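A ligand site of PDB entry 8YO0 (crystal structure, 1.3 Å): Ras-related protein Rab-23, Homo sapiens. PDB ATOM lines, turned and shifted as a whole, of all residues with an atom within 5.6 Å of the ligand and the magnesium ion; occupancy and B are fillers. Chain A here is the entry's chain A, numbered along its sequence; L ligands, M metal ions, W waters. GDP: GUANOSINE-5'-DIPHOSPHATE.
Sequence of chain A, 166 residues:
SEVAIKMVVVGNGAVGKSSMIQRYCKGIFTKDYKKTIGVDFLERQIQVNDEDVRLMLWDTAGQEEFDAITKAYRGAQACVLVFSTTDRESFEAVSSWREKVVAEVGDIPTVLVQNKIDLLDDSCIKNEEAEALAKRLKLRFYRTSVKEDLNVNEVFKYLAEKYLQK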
ATOM      1  N   ASN A  12       2.067 -21.713  12.282  1.00  0.00           N
ATOM      2  CA  ASN A  12       0.736 -21.384  11.767  1.00  0.00           C
ATOM      3  C   ASN A  12       0.208 -20.077  12.362  1.00  0.00           C
ATOM      4  O   ASN A  12       0.694 -19.567  13.386  1.00  0.00           O
ATOM      5  CB  ASN A  12      -0.263 -22.502  12.074  1.00  0.00           C
ATOM      6  CG  ASN A  12      -0.217 -23.621  11.070  1.00  0.00           C
ATOM      7  OD1 ASN A  12       0.736 -23.759  10.318  1.00  0.00           O
ATOM      8  ND2 ASN A  12      -1.290 -24.408  11.015  1.00  0.00           N
ATOM      9  N   GLY A  13      -0.827 -19.545  11.721  1.00  0.00           N
ATOM     10  CA  GLY A  13      -1.468 -18.336  12.226  1.00  0.00           C
ATOM     11  C   GLY A  13      -2.039 -18.529  13.624  1.00  0.00           C
ATOM     12  O   GLY A  13      -2.525 -19.604  13.990  1.00  0.00           O
ATOM     13  N   ALA A  14      -1.952 -17.458  14.408  1.00  0.00           N
ATOM     14  CA  ALA A  14      -2.562 -17.340  15.728  1.00  0.00           C
ATOM     15  C   ALA A  14      -1.848 -18.132  16.812  1.00  0.00           C
ATOM     16  O   ALA A  14      -2.354 -18.175  17.952  1.00  0.00           O
ATOM     17  CB  ALA A  14      -4.074 -17.580  15.729  1.00  0.00           C
ATOM     18  N   VAL A  15      -0.672 -18.703  16.533  1.00  0.00           N
ATOM     19  CA  VAL A  15       0.019 -19.437  17.580  1.00  0.00           C
ATOM     20  C   VAL A  15       0.711 -18.513  18.568  1.00  0.00           C
ATOM     21  O   VAL A  15       1.069 -18.965  19.669  1.00  0.00           O
ATOM     22  CB  VAL A  15       1.028 -20.459  17.016  1.00  0.00           C
ATOM     23  CG1 VAL A  15       0.312 -21.462  16.100  1.00  0.00           C
ATOM     24  CG2 VAL A  15       2.207 -19.785  16.285  1.00  0.00           C
ATOM     25  N   GLY A  16       0.906 -17.240  18.196  1.00  0.00           N
ATOM     26  CA  GLY A  16       1.552 -16.268  19.066  1.00  0.00           C
ATOM     27  C   GLY A  16       2.887 -15.766  18.595  1.00  0.00           C
ATOM     28  O   GLY A  16       3.647 -15.226  19.435  1.00  0.00           O
ATOM     29  N   LYS A  17       3.190 -15.828  17.306  1.00  0.00           N
ATOM     30  CA  LYS A  17       4.505 -15.391  16.813  1.00  0.00           C
ATOM     31  C   LYS A  17       4.725 -13.904  17.040  1.00  0.00           C
ATOM     32  O   LYS A  17       5.756 -13.486  17.594  1.00  0.00           O
ATOM     33  CB  LYS A  17       4.642 -15.728  15.320  1.00  0.00           C
ATOM     34  CG  LYS A  17       4.514 -17.200  15.073  1.00  0.00           C
ATOM     35  CD  LYS A  17       4.718 -17.555  13.576  1.00  0.00           C
ATOM     36  CE  LYS A  17       3.751 -16.839  12.648  1.00  0.00           C
ATOM     37  NZ  LYS A  17       2.323 -17.199  12.888  1.00  0.00           N
ATOM     38  N   SER A  18       3.770 -13.081  16.617  1.00  0.00           N
ATOM     39  CA  SER A  18       3.974 -11.644  16.728  1.00  0.00           C
ATOM     40  C   SER A  18       4.027 -11.259  18.196  1.00  0.00           C
ATOM     41  O   SER A  18       4.857 -10.420  18.601  1.00  0.00           O
ATOM     42  CB  SER A  18       2.827 -10.931  16.031  1.00  0.00           C
ATOM     43  OG  SER A  18       2.791 -11.259  14.662  1.00  0.00           O
ATOM     44  N   SER A  19       3.169 -11.862  19.016  1.00  0.00           N
ATOM     45  CA  SER A  19       3.201 -11.599  20.452  1.00  0.00           C
ATOM     46  C   SER A  19       4.528 -11.987  21.056  1.00  0.00           C
ATOM     47  O   SER A  19       5.065 -11.260  21.909  1.00  0.00           O
ATOM     48  CB  SER A  19       2.096 -12.392  21.159  1.00  0.00           C
ATOM     49  OG  SER A  19       0.767 -11.979  20.739  1.00  0.00           O
ATOM     50  N   MET A  20       5.067 -13.138  20.641  1.00  0.00           N
ATOM     51  CA  MET A  20       6.342 -13.556  21.190  1.00  0.00           C
ATOM     52  C   MET A  20       7.442 -12.557  20.906  1.00  0.00           C
ATOM     53  O   MET A  20       8.243 -12.217  21.799  1.00  0.00           O
ATOM     54  CB  MET A  20       6.689 -14.926  20.633  1.00  0.00           C
ATOM     55  CG  MET A  20       7.953 -15.493  21.228  1.00  0.00           C
ATOM     56  SD  MET A  20       8.339 -17.129  20.549  1.00  0.00           S
ATOM     57  CE  MET A  20       6.911 -18.093  21.090  1.00  0.00           C
ATOM     58  N   PHE A  29       2.668  -7.174  26.355  1.00  0.00           N
ATOM     59  CA  PHE A  29       1.670  -8.127  25.884  1.00  0.00           C
ATOM     60  C   PHE A  29       0.331  -7.423  25.888  1.00  0.00           C
ATOM     61  O   PHE A  29      -0.208  -7.162  26.961  1.00  0.00           O
ATOM     62  CB  PHE A  29       1.599  -9.383  26.765  1.00  0.00           C
ATOM     63  CG  PHE A  29       0.579 -10.408  26.288  1.00  0.00           C
ATOM     64  CD1 PHE A  29       0.873 -11.250  25.225  1.00  0.00           C
ATOM     65  CD2 PHE A  29      -0.664 -10.521  26.904  1.00  0.00           C
ATOM     66  CE1 PHE A  29      -0.052 -12.204  24.800  1.00  0.00           C
ATOM     67  CE2 PHE A  29      -1.583 -11.464  26.472  1.00  0.00           C
ATOM     68  CZ  PHE A  29      -1.261 -12.308  25.418  1.00  0.00           C
ATOM     69  N   THR A  30      -0.206  -7.121  24.718  1.00  0.00           N
ATOM     70  CA  THR A  30      -1.477  -6.416  24.637  1.00  0.00           C
ATOM     71  C   THR A  30      -2.633  -7.414  24.452  1.00  0.00           C
ATOM     72  O   THR A  30      -2.418  -8.622  24.272  1.00  0.00           O
ATOM     73  CB  THR A  30      -1.429  -5.394  23.506  1.00  0.00           C
ATOM     74  OG1 THR A  30      -1.345  -6.067  22.250  1.00  0.00           O
ATOM     75  CG2 THR A  30      -0.222  -4.488  23.668  1.00  0.00           C
ATOM     76  N   LYS A  31      -3.869  -6.914  24.516  1.00  0.00           N
ATOM     77  CA  LYS A  31      -5.037  -7.797  24.567  1.00  0.00           C
ATOM     78  C   LYS A  31      -5.714  -7.993  23.215  1.00  0.00           C
ATOM     79  O   LYS A  31      -6.813  -8.551  23.159  1.00  0.00           O
ATOM     80  CB  LYS A  31      -6.029  -7.334  25.634  1.00  0.00           C
ATOM     81  N   ASP A  32      -5.073  -7.556  22.134  1.00  0.00           N
ATOM     82  CA  ASP A  32      -5.654  -7.637  20.803  1.00  0.00           C
ATOM     83  C   ASP A  32      -5.838  -9.072  20.339  1.00  0.00           C
ATOM     84  O   ASP A  32      -5.091  -9.986  20.730  1.00  0.00           O
ATOM     85  CB  ASP A  32      -4.732  -6.919  19.824  1.00  0.00           C
ATOM     86  CG  ASP A  32      -4.453  -5.494  20.254  1.00  0.00           C
ATOM     87  OD1 ASP A  32      -5.295  -4.632  19.972  1.00  0.00           O
ATOM     88  OD2 ASP A  32      -3.427  -5.253  20.901  1.00  0.00           O
ATOM     89  N   TYR A  33      -6.847  -9.267  19.480  1.00  0.00           N
ATOM     90  CA  TYR A  33      -7.100 -10.582  18.904  1.00  0.00           C
ATOM     91  C   TYR A  33      -5.975 -10.986  17.958  1.00  0.00           C
ATOM     92  O   TYR A  33      -5.671 -12.187  17.837  1.00  0.00           O
ATOM     93  CB  TYR A  33      -8.449 -10.581  18.177  1.00  0.00           C
ATOM     94  N   LYS A  34      -5.331 -10.016  17.310  1.00  0.00           N
ATOM     95  CA  LYS A  34      -4.243 -10.242  16.379  1.00  0.00           C
ATOM     96  C   LYS A  34      -3.207  -9.132  16.567  1.00  0.00           C
ATOM     97  O   LYS A  34      -3.563  -7.953  16.554  1.00  0.00           O
ATOM     98  CB  LYS A  34      -4.779 -10.252  14.931  1.00  0.00           C
ATOM     99  CG  LYS A  34      -3.705 -10.396  13.862  1.00  0.00           C
ATOM    100  N   LYS A  35      -1.949  -9.519  16.782  1.00  0.00           N
ATOM    101  CA  LYS A  35      -0.902  -8.522  16.977  1.00  0.00           C
ATOM    102  C   LYS A  35      -0.321  -8.132  15.620  1.00  0.00           C
ATOM    103  O   LYS A  35      -0.466  -8.852  14.627  1.00  0.00           O
ATOM    104  CB  LYS A  35       0.180  -9.065  17.925  1.00  0.00           C
ATOM    105  CG  LYS A  35      -0.163  -8.910  19.439  1.00  0.00           C
ATOM    106  CD  LYS A  35      -1.444  -9.654  19.817  1.00  0.00           C
ATOM    107  CE  LYS A  35      -1.897  -9.385  21.229  1.00  0.00           C
ATOM    108  NZ  LYS A  35      -0.997  -9.990  22.254  1.00  0.00           N
ATOM    109  N   ASP A  59       9.350 -11.646  12.024  1.00  0.00           N
ATOM    110  CA  ASP A  59       8.026 -12.225  12.036  1.00  0.00           C
ATOM    111  C   ASP A  59       7.690 -12.778  10.659  1.00  0.00           C
ATOM    112  O   ASP A  59       8.279 -12.397   9.643  1.00  0.00           O
ATOM    113  CB  ASP A  59       7.038 -11.125  12.421  1.00  0.00           C
ATOM    114  CG  ASP A  59       5.740 -11.648  13.040  1.00  0.00           C
ATOM    115  OD1 ASP A  59       5.542 -12.874  13.185  1.00  0.00           O
ATOM    116  OD2 ASP A  59       4.920 -10.765  13.394  1.00  0.00           O
ATOM    117  N   THR A  60       6.726 -13.721  10.639  1.00  0.00           N
ATOM    118  CA  THR A  60       6.306 -14.366   9.409  1.00  0.00           C
ATOM    119  C   THR A  60       4.791 -14.461   9.360  1.00  0.00           C
ATOM    120  O   THR A  60       4.094 -14.241  10.352  1.00  0.00           O
ATOM    121  CB  THR A  60       6.868 -15.790   9.272  1.00  0.00           C
ATOM    122  OG1 THR A  60       6.419 -16.578  10.392  1.00  0.00           O
ATOM    123  CG2 THR A  60       8.393 -15.820   9.224  1.00  0.00           C
ATOM    124  N   ASN A 115       3.464 -22.818  22.573  1.00  0.00           N
ATOM    125  CA  ASN A 115       3.057 -21.588  23.211  1.00  0.00           C
ATOM    126  C   ASN A 115       1.661 -21.762  23.814  1.00  0.00           C
ATOM    127  O   ASN A 115       0.950 -22.739  23.565  1.00  0.00           O
ATOM    128  CB  ASN A 115       3.126 -20.422  22.213  1.00  0.00           C
ATOM    129  CG  ASN A 115       2.946 -19.086  22.877  1.00  0.00           C
ATOM    130  OD1 ASN A 115       3.430 -18.860  23.991  1.00  0.00           O
ATOM    131  ND2 ASN A 115       2.219 -18.188  22.214  1.00  0.00           N
ATOM    132  N   LYS A 116       1.270 -20.750  24.599  1.00  0.00           N
ATOM    133  CA  LYS A 116      -0.037 -20.702  25.264  1.00  0.00           C
ATOM    134  C   LYS A 116      -0.188 -21.816  26.283  1.00  0.00           C
ATOM    135  O   LYS A 116      -1.284 -22.318  26.505  1.00  0.00           O
ATOM    136  CB  LYS A 116      -1.236 -20.688  24.294  1.00  0.00           C
ATOM    137  CG  LYS A 116      -1.066 -19.769  23.082  1.00  0.00           C
ATOM    138  CD  LYS A 116      -2.389 -19.493  22.391  1.00  0.00           C
ATOM    139  CE  LYS A 116      -2.207 -18.634  21.151  1.00  0.00           C
ATOM    140  NZ  LYS A 116      -3.503 -18.395  20.425  1.00  0.00           N
ATOM    141  N   ILE A 117       0.906 -22.159  26.968  1.00  0.00           N
ATOM    142  CA  ILE A 117       0.844 -23.219  27.989  1.00  0.00           C
ATOM    143  C   ILE A 117      -0.019 -22.789  29.160  1.00  0.00           C
ATOM    144  O   ILE A 117      -0.462 -23.651  29.933  1.00  0.00           O
ATOM    145  CB  ILE A 117       2.269 -23.686  28.370  1.00  0.00           C
ATOM    146  CG1 ILE A 117       2.247 -25.112  28.910  1.00  0.00           C
ATOM    147  CG2 ILE A 117       2.909 -22.759  29.408  1.00  0.00           C
ATOM    148  CD1 ILE A 117       1.888 -26.094  27.794  1.00  0.00           C
ATOM    149  N   ASP A 118      -0.295 -21.500  29.301  1.00  0.00           N
ATOM    150  CA  ASP A 118      -1.252 -21.063  30.325  1.00  0.00           C
ATOM    151  C   ASP A 118      -2.666 -21.573  30.040  1.00  0.00           C
ATOM    152  O   ASP A 118      -3.524 -21.547  30.949  1.00  0.00           O
ATOM    153  CB  ASP A 118      -1.240 -19.529  30.412  1.00  0.00           C
ATOM    154  CG  ASP A 118      -1.565 -18.867  29.067  1.00  0.00           C
ATOM    155  OD1 ASP A 118      -0.707 -18.878  28.139  1.00  0.00           O
ATOM    156  OD2 ASP A 118      -2.699 -18.331  28.926  1.00  0.00           O
ATOM    157  N   LEU A 119      -2.921 -22.048  28.817  1.00  0.00           N
ATOM    158  CA  LEU A 119      -4.209 -22.620  28.443  1.00  0.00           C
ATOM    159  C   LEU A 119      -4.214 -24.142  28.493  1.00  0.00           C
ATOM    160  O   LEU A 119      -4.975 -24.803  27.779  1.00  0.00           O
ATOM    161  CB  LEU A 119      -4.602 -22.154  27.037  1.00  0.00           C
ATOM    162  CG  LEU A 119      -4.640 -20.638  26.830  1.00  0.00           C
ATOM    163  CD1 LEU A 119      -5.056 -20.328  25.385  1.00  0.00           C
ATOM    164  CD2 LEU A 119      -5.529 -19.920  27.841  1.00  0.00           C
ATOM    165  N   THR A 144       5.985 -22.562  26.500  1.00  0.00           N
ATOM    166  CA  THR A 144       6.047 -21.134  26.727  1.00  0.00           C
ATOM    167  C   THR A 144       4.642 -20.576  26.965  1.00  0.00           C
ATOM    168  O   THR A 144       3.654 -21.113  26.476  1.00  0.00           O
ATOM    169  CB  THR A 144       6.700 -20.501  25.505  1.00  0.00           C
ATOM    170  OG1 THR A 144       8.080 -20.874  25.467  1.00  0.00           O
ATOM    171  CG2 THR A 144       6.605 -19.043  25.536  1.00  0.00           C
ATOM    172  N   SER A 145       4.582 -19.497  27.715  1.00  0.00           N
ATOM    173  CA  SER A 145       3.405 -18.626  27.718  1.00  0.00           C
ATOM    174  C   SER A 145       3.908 -17.205  27.482  1.00  0.00           C
ATOM    175  O   SER A 145       4.520 -16.599  28.373  1.00  0.00           O
ATOM    176  CB  SER A 145       2.622 -18.673  29.020  1.00  0.00           C
ATOM    177  OG  SER A 145       1.602 -17.668  28.989  1.00  0.00           O
ATOM    178  N   VAL A 146       3.698 -16.684  26.284  1.00  0.00           N
ATOM    179  CA  VAL A 146       4.026 -15.285  26.042  1.00  0.00           C
ATOM    180  C   VAL A 146       3.215 -14.399  26.985  1.00  0.00           C
ATOM    181  O   VAL A 146       3.724 -13.378  27.493  1.00  0.00           O
ATOM    182  CB  VAL A 146       3.752 -14.941  24.566  1.00  0.00           C
ATOM    183  CG1 VAL A 146       3.967 -13.436  24.338  1.00  0.00           C
ATOM    184  CG2 VAL A 146       4.624 -15.782  23.655  1.00  0.00           C
ATOM    185  N   LYS A 147       1.966 -14.771  27.256  1.00  0.00           N
ATOM    186  CA  LYS A 147       1.104 -13.960  28.102  1.00  0.00           C
ATOM    187  C   LYS A 147       1.699 -13.832  29.503  1.00  0.00           C
ATOM    188  O   LYS A 147       1.684 -12.740  30.089  1.00  0.00           O
ATOM    189  CB  LYS A 147      -0.287 -14.603  28.130  1.00  0.00           C
ATOM    190  CG  LYS A 147      -1.262 -13.896  29.069  1.00  0.00           C
ATOM    191  CD  LYS A 147      -2.627 -14.573  29.038  1.00  0.00           C
ATOM    192  CE  LYS A 147      -3.598 -13.916  30.021  1.00  0.00           C
ATOM    193  NZ  LYS A 147      -4.959 -14.505  29.924  1.00  0.00           N
ATOM    194  N   GLU A 148       2.254 -14.923  30.025  1.00  0.00           N
ATOM    195  CA  GLU A 148       2.849 -14.942  31.370  1.00  0.00           C
ATOM    196  C   GLU A 148       4.341 -14.649  31.381  1.00  0.00           C
ATOM    197  O   GLU A 148       4.965 -14.728  32.443  1.00  0.00           O
ATOM    198  CB  GLU A 148       2.622 -16.324  32.000  1.00  0.00           C
ATOM    199  CG  GLU A 148       1.159 -16.613  32.288  1.00  0.00           C
ATOM    200  CD  GLU A 148       0.930 -18.006  32.852  1.00  0.00           C
ATOM    201  OE1 GLU A 148       1.849 -18.859  32.759  1.00  0.00           O
ATOM    202  OE2 GLU A 148      -0.163 -18.252  33.373  1.00  0.00           O
HETATM  203  PB  GDP L   1       0.472 -14.952  15.260  1.00  0.00           P
HETATM  204  O1B GDP L   1      -0.671 -14.998  14.261  1.00  0.00           O
HETATM  205  O2B GDP L   1       1.188 -16.279  15.387  1.00  0.00           O
HETATM  206  O3B GDP L   1       1.391 -13.772  15.042  1.00  0.00           O
HETATM  207  O3A GDP L   1      -0.212 -14.741  16.663  1.00  0.00           O
HETATM  208  PA  GDP L   1      -0.509 -13.451  17.544  1.00  0.00           P
HETATM  209  O1A GDP L   1      -1.271 -12.481  16.723  1.00  0.00           O
HETATM  210  O2A GDP L   1       0.737 -12.988  18.219  1.00  0.00           O
HETATM  211  O5' GDP L   1      -1.399 -14.009  18.701  1.00  0.00           O
HETATM  212  C5' GDP L   1      -2.702 -14.572  18.404  1.00  0.00           C
HETATM  213  C4' GDP L   1      -3.561 -14.473  19.646  1.00  0.00           C
HETATM  214  O4' GDP L   1      -3.006 -15.328  20.685  1.00  0.00           O
HETATM  215  C3' GDP L   1      -3.611 -13.063  20.245  1.00  0.00           C
HETATM  216  O3' GDP L   1      -4.879 -12.791  20.839  1.00  0.00           O
HETATM  217  C2' GDP L   1      -2.570 -13.162  21.374  1.00  0.00           C
HETATM  218  O2' GDP L   1      -2.761 -12.239  22.445  1.00  0.00           O
HETATM  219  C1' GDP L   1      -2.795 -14.578  21.860  1.00  0.00           C
HETATM  220  N9  GDP L   1      -1.641 -15.141  22.586  1.00  0.00           N
HETATM  221  C8  GDP L   1      -0.329 -15.105  22.186  1.00  0.00           C
HETATM  222  N7  GDP L   1       0.456 -15.731  23.026  1.00  0.00           N
HETATM  223  C5  GDP L   1      -0.382 -16.199  24.019  1.00  0.00           C
HETATM  224  C6  GDP L   1      -0.108 -16.942  25.183  1.00  0.00           C
HETATM  225  O6  GDP L   1       0.990 -17.324  25.603  1.00  0.00           O
HETATM  226  N1  GDP L   1      -1.248 -17.201  25.905  1.00  0.00           N
HETATM  227  C2  GDP L   1      -2.509 -16.816  25.583  1.00  0.00           C
HETATM  228  N2  GDP L   1      -3.485 -17.154  26.447  1.00  0.00           N
HETATM  229  N3  GDP L   1      -2.794 -16.105  24.499  1.00  0.00           N
HETATM  230  C4  GDP L   1      -1.684 -15.836  23.764  1.00  0.00           C
HETATM  231 MG    MG M   1       1.411 -12.366  13.575  1.00  0.00          MG
HETATM  232  O   HOH W   1      -4.973 -17.157  22.648  1.00  0.00           O
HETATM  233  O   HOH W   2       0.092 -13.430  12.376  1.00  0.00           O
HETATM  234  O   HOH W   3      -5.032 -12.080  23.818  1.00  0.00           O
HETATM  235  O   HOH W   4      -0.236 -11.463  14.484  1.00  0.00           O
HETATM  236  O   HOH W   5       2.998 -13.340  12.694  1.00  0.00           O
HETATM  237  O   HOH W   6      -3.271 -14.113  14.288  1.00  0.00           O
HETATM  238  O   HOH W   7       1.380 -10.854  12.150  1.00  0.00           O
HETATM  239  O   HOH W   8      -7.294 -11.066  22.660  1.00  0.00           O
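An oxygen (O2A) of the ligand is in hydrogen-bond range of the backbone NH (N) of Ser 18, at 3.4 Å. N of Ser 19 is in hydrogen-bond range of O2A of the ligand, 2.8 Å away. OG of Ser 19 is in hydrogen-bond range of O2A of the ligand. The backbone NH of Ala 14 sits at hydrogen-bond distance from an oxygen (O1B) of the ligand, at 2.8 Å. N of Lys 17 is in hydrogen-bond range of O2B of the ligand (2.8 Å). The side-chain amino group (NZ) of Lys 17 is in salt-bridge range of an oxygen (O2B) of the ligand, 2.9 Å away. O3' of the ligand sits at hydrogen-bond distance from O of Asp 32, at 2.8 Å. The side-chain carboxylate (OD1) of Asp 118 lies within hydrogen-bond range of a nitrogen (N1) of the ligand. The backbone NH (N) of Val 146 sits at hydrogen-bond distance from an oxygen (O6) of the ligand (2.9 Å). An oxygen (O1A) of the ligand sits at hydrogen-bond distance from the backbone NH (N) of Lys 35, 3.0 Å away. The side-chain amino group (NZ) of Lys 35 is in hydrogen-bond range of an oxygen (O2') of the ligand (2.9 Å). An oxygen (O2B) of the ligand is in hydrogen-bond range of the backbone NH of Gly 16 (3.0 Å). The side-chain amino group (NZ) of Lys 116 lies within hydrogen-bond range of an oxygen (O4') of the ligand (3.1 Å). ND2 of Asn 115 lies within hydrogen-bond range of N7 of the ligand (3.1 Å). An oxygen (O3') of the ligand lies within hydrogen-bond range of the backbone carbonyl oxygen of Tyr 33 (3.2 Å). O6 of the ligand sits at hydrogen-bond distance from N of Lys 147, 3.2 Å away. An oxygen (O2B) of the ligand sits at hydrogen-bond distance from the backbone NH of Val 15. OG of Ser 145 sits at hydrogen-bond distance from O6 of the ligand (3.5 Å).
The side-chain hydroxyl of Ser 19 lies within hydrogen-bond range of the side-chain amino group of Lys 35. The backbone carbonyl oxygen (O) of Ala 14 is in hydrogen-bond range of the side-chain amino group (NZ) of Lys 116 (2.7 Å). OD1 of Asp 118 sits at hydrogen-bond distance from OG of Ser 145. The backbone NH of Val 146 lies within hydrogen-bond range of the side-chain amide oxygen of Asn 115, at 3.2 Å. O of Thr 30 sits at hydrogen-bond distance from NZ of Lys 35 (2.8 Å). The side-chain amide nitrogen (ND2) of Asn 115 sits at hydrogen-bond distance from the backbone carbonyl oxygen (O) of Val 15, 2.9 Å away. OD1 of Asn 115 sits close to O of Thr 144. The side-chain hydroxyl (OG) of Ser 145 is in hydrogen-bond range of the backbone NH (N) of Glu 148 (3.0 Å).
O of Asn 12 touches O2B of the ligand, at 3.9 Å. Gly 13 touches the ligand. CZ of Phe 29 touches O2' of the ligand, at 3.3 Å. Lys 34 touches the ligand. Leu 119 touches the ligand (CG to N2, 3.7 Å). Hydrophobic or aromatic side chains that line the ligand: Val 15, Phe 29, Leu 119 and Val 146. 20 residues have an atom within 4 Å of the ligand: Asn 12, Gly 13, Ala 14, Val 15, Gly 16, Lys 17, Ser 18, Ser 19, Phe 29, Asp 32, Tyr 33, Lys 34, Lys 35, Asn 115, Lys 116, Asp 118, Leu 119, Ser 145, Val 146 and Lys 147.
Asp 59 touches the magnesium ion. Within 4 Å of the magnesium ion: Ser 18 and Asp 59.
The magnesium ion is bound by an oxygen (O3B) of the ligand (2.0 Å), water W5 (2.1 Å), water W2 (2.1 Å), the side-chain hydroxyl (OG) of Ser 18 (2.1 Å), water W7 (2.1 Å) and water W4 (2.1 Å). The magnesium ion has six donor atoms within binding distance.
Water W4 lies within hydrogen-bond range of O of Lys 35 and O1A of the ligand. Water W5 bridges the side-chain carboxylate (OD1) of Asp 59 (2.6 Å) and the backbone carbonyl oxygen (O) of Thr 60 (2.7 Å). Water W1 bridges the side-chain amino group (NZ) of Lys 116 (2.9 Å) and a nitrogen (N3) of the ligand (3.0 Å). Water W8 lies within hydrogen-bond range of the backbone carbonyl oxygen (O) of Lys 31, the backbone carbonyl oxygen (O) of Asp 32 and an oxygen (O3') of the ligand.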
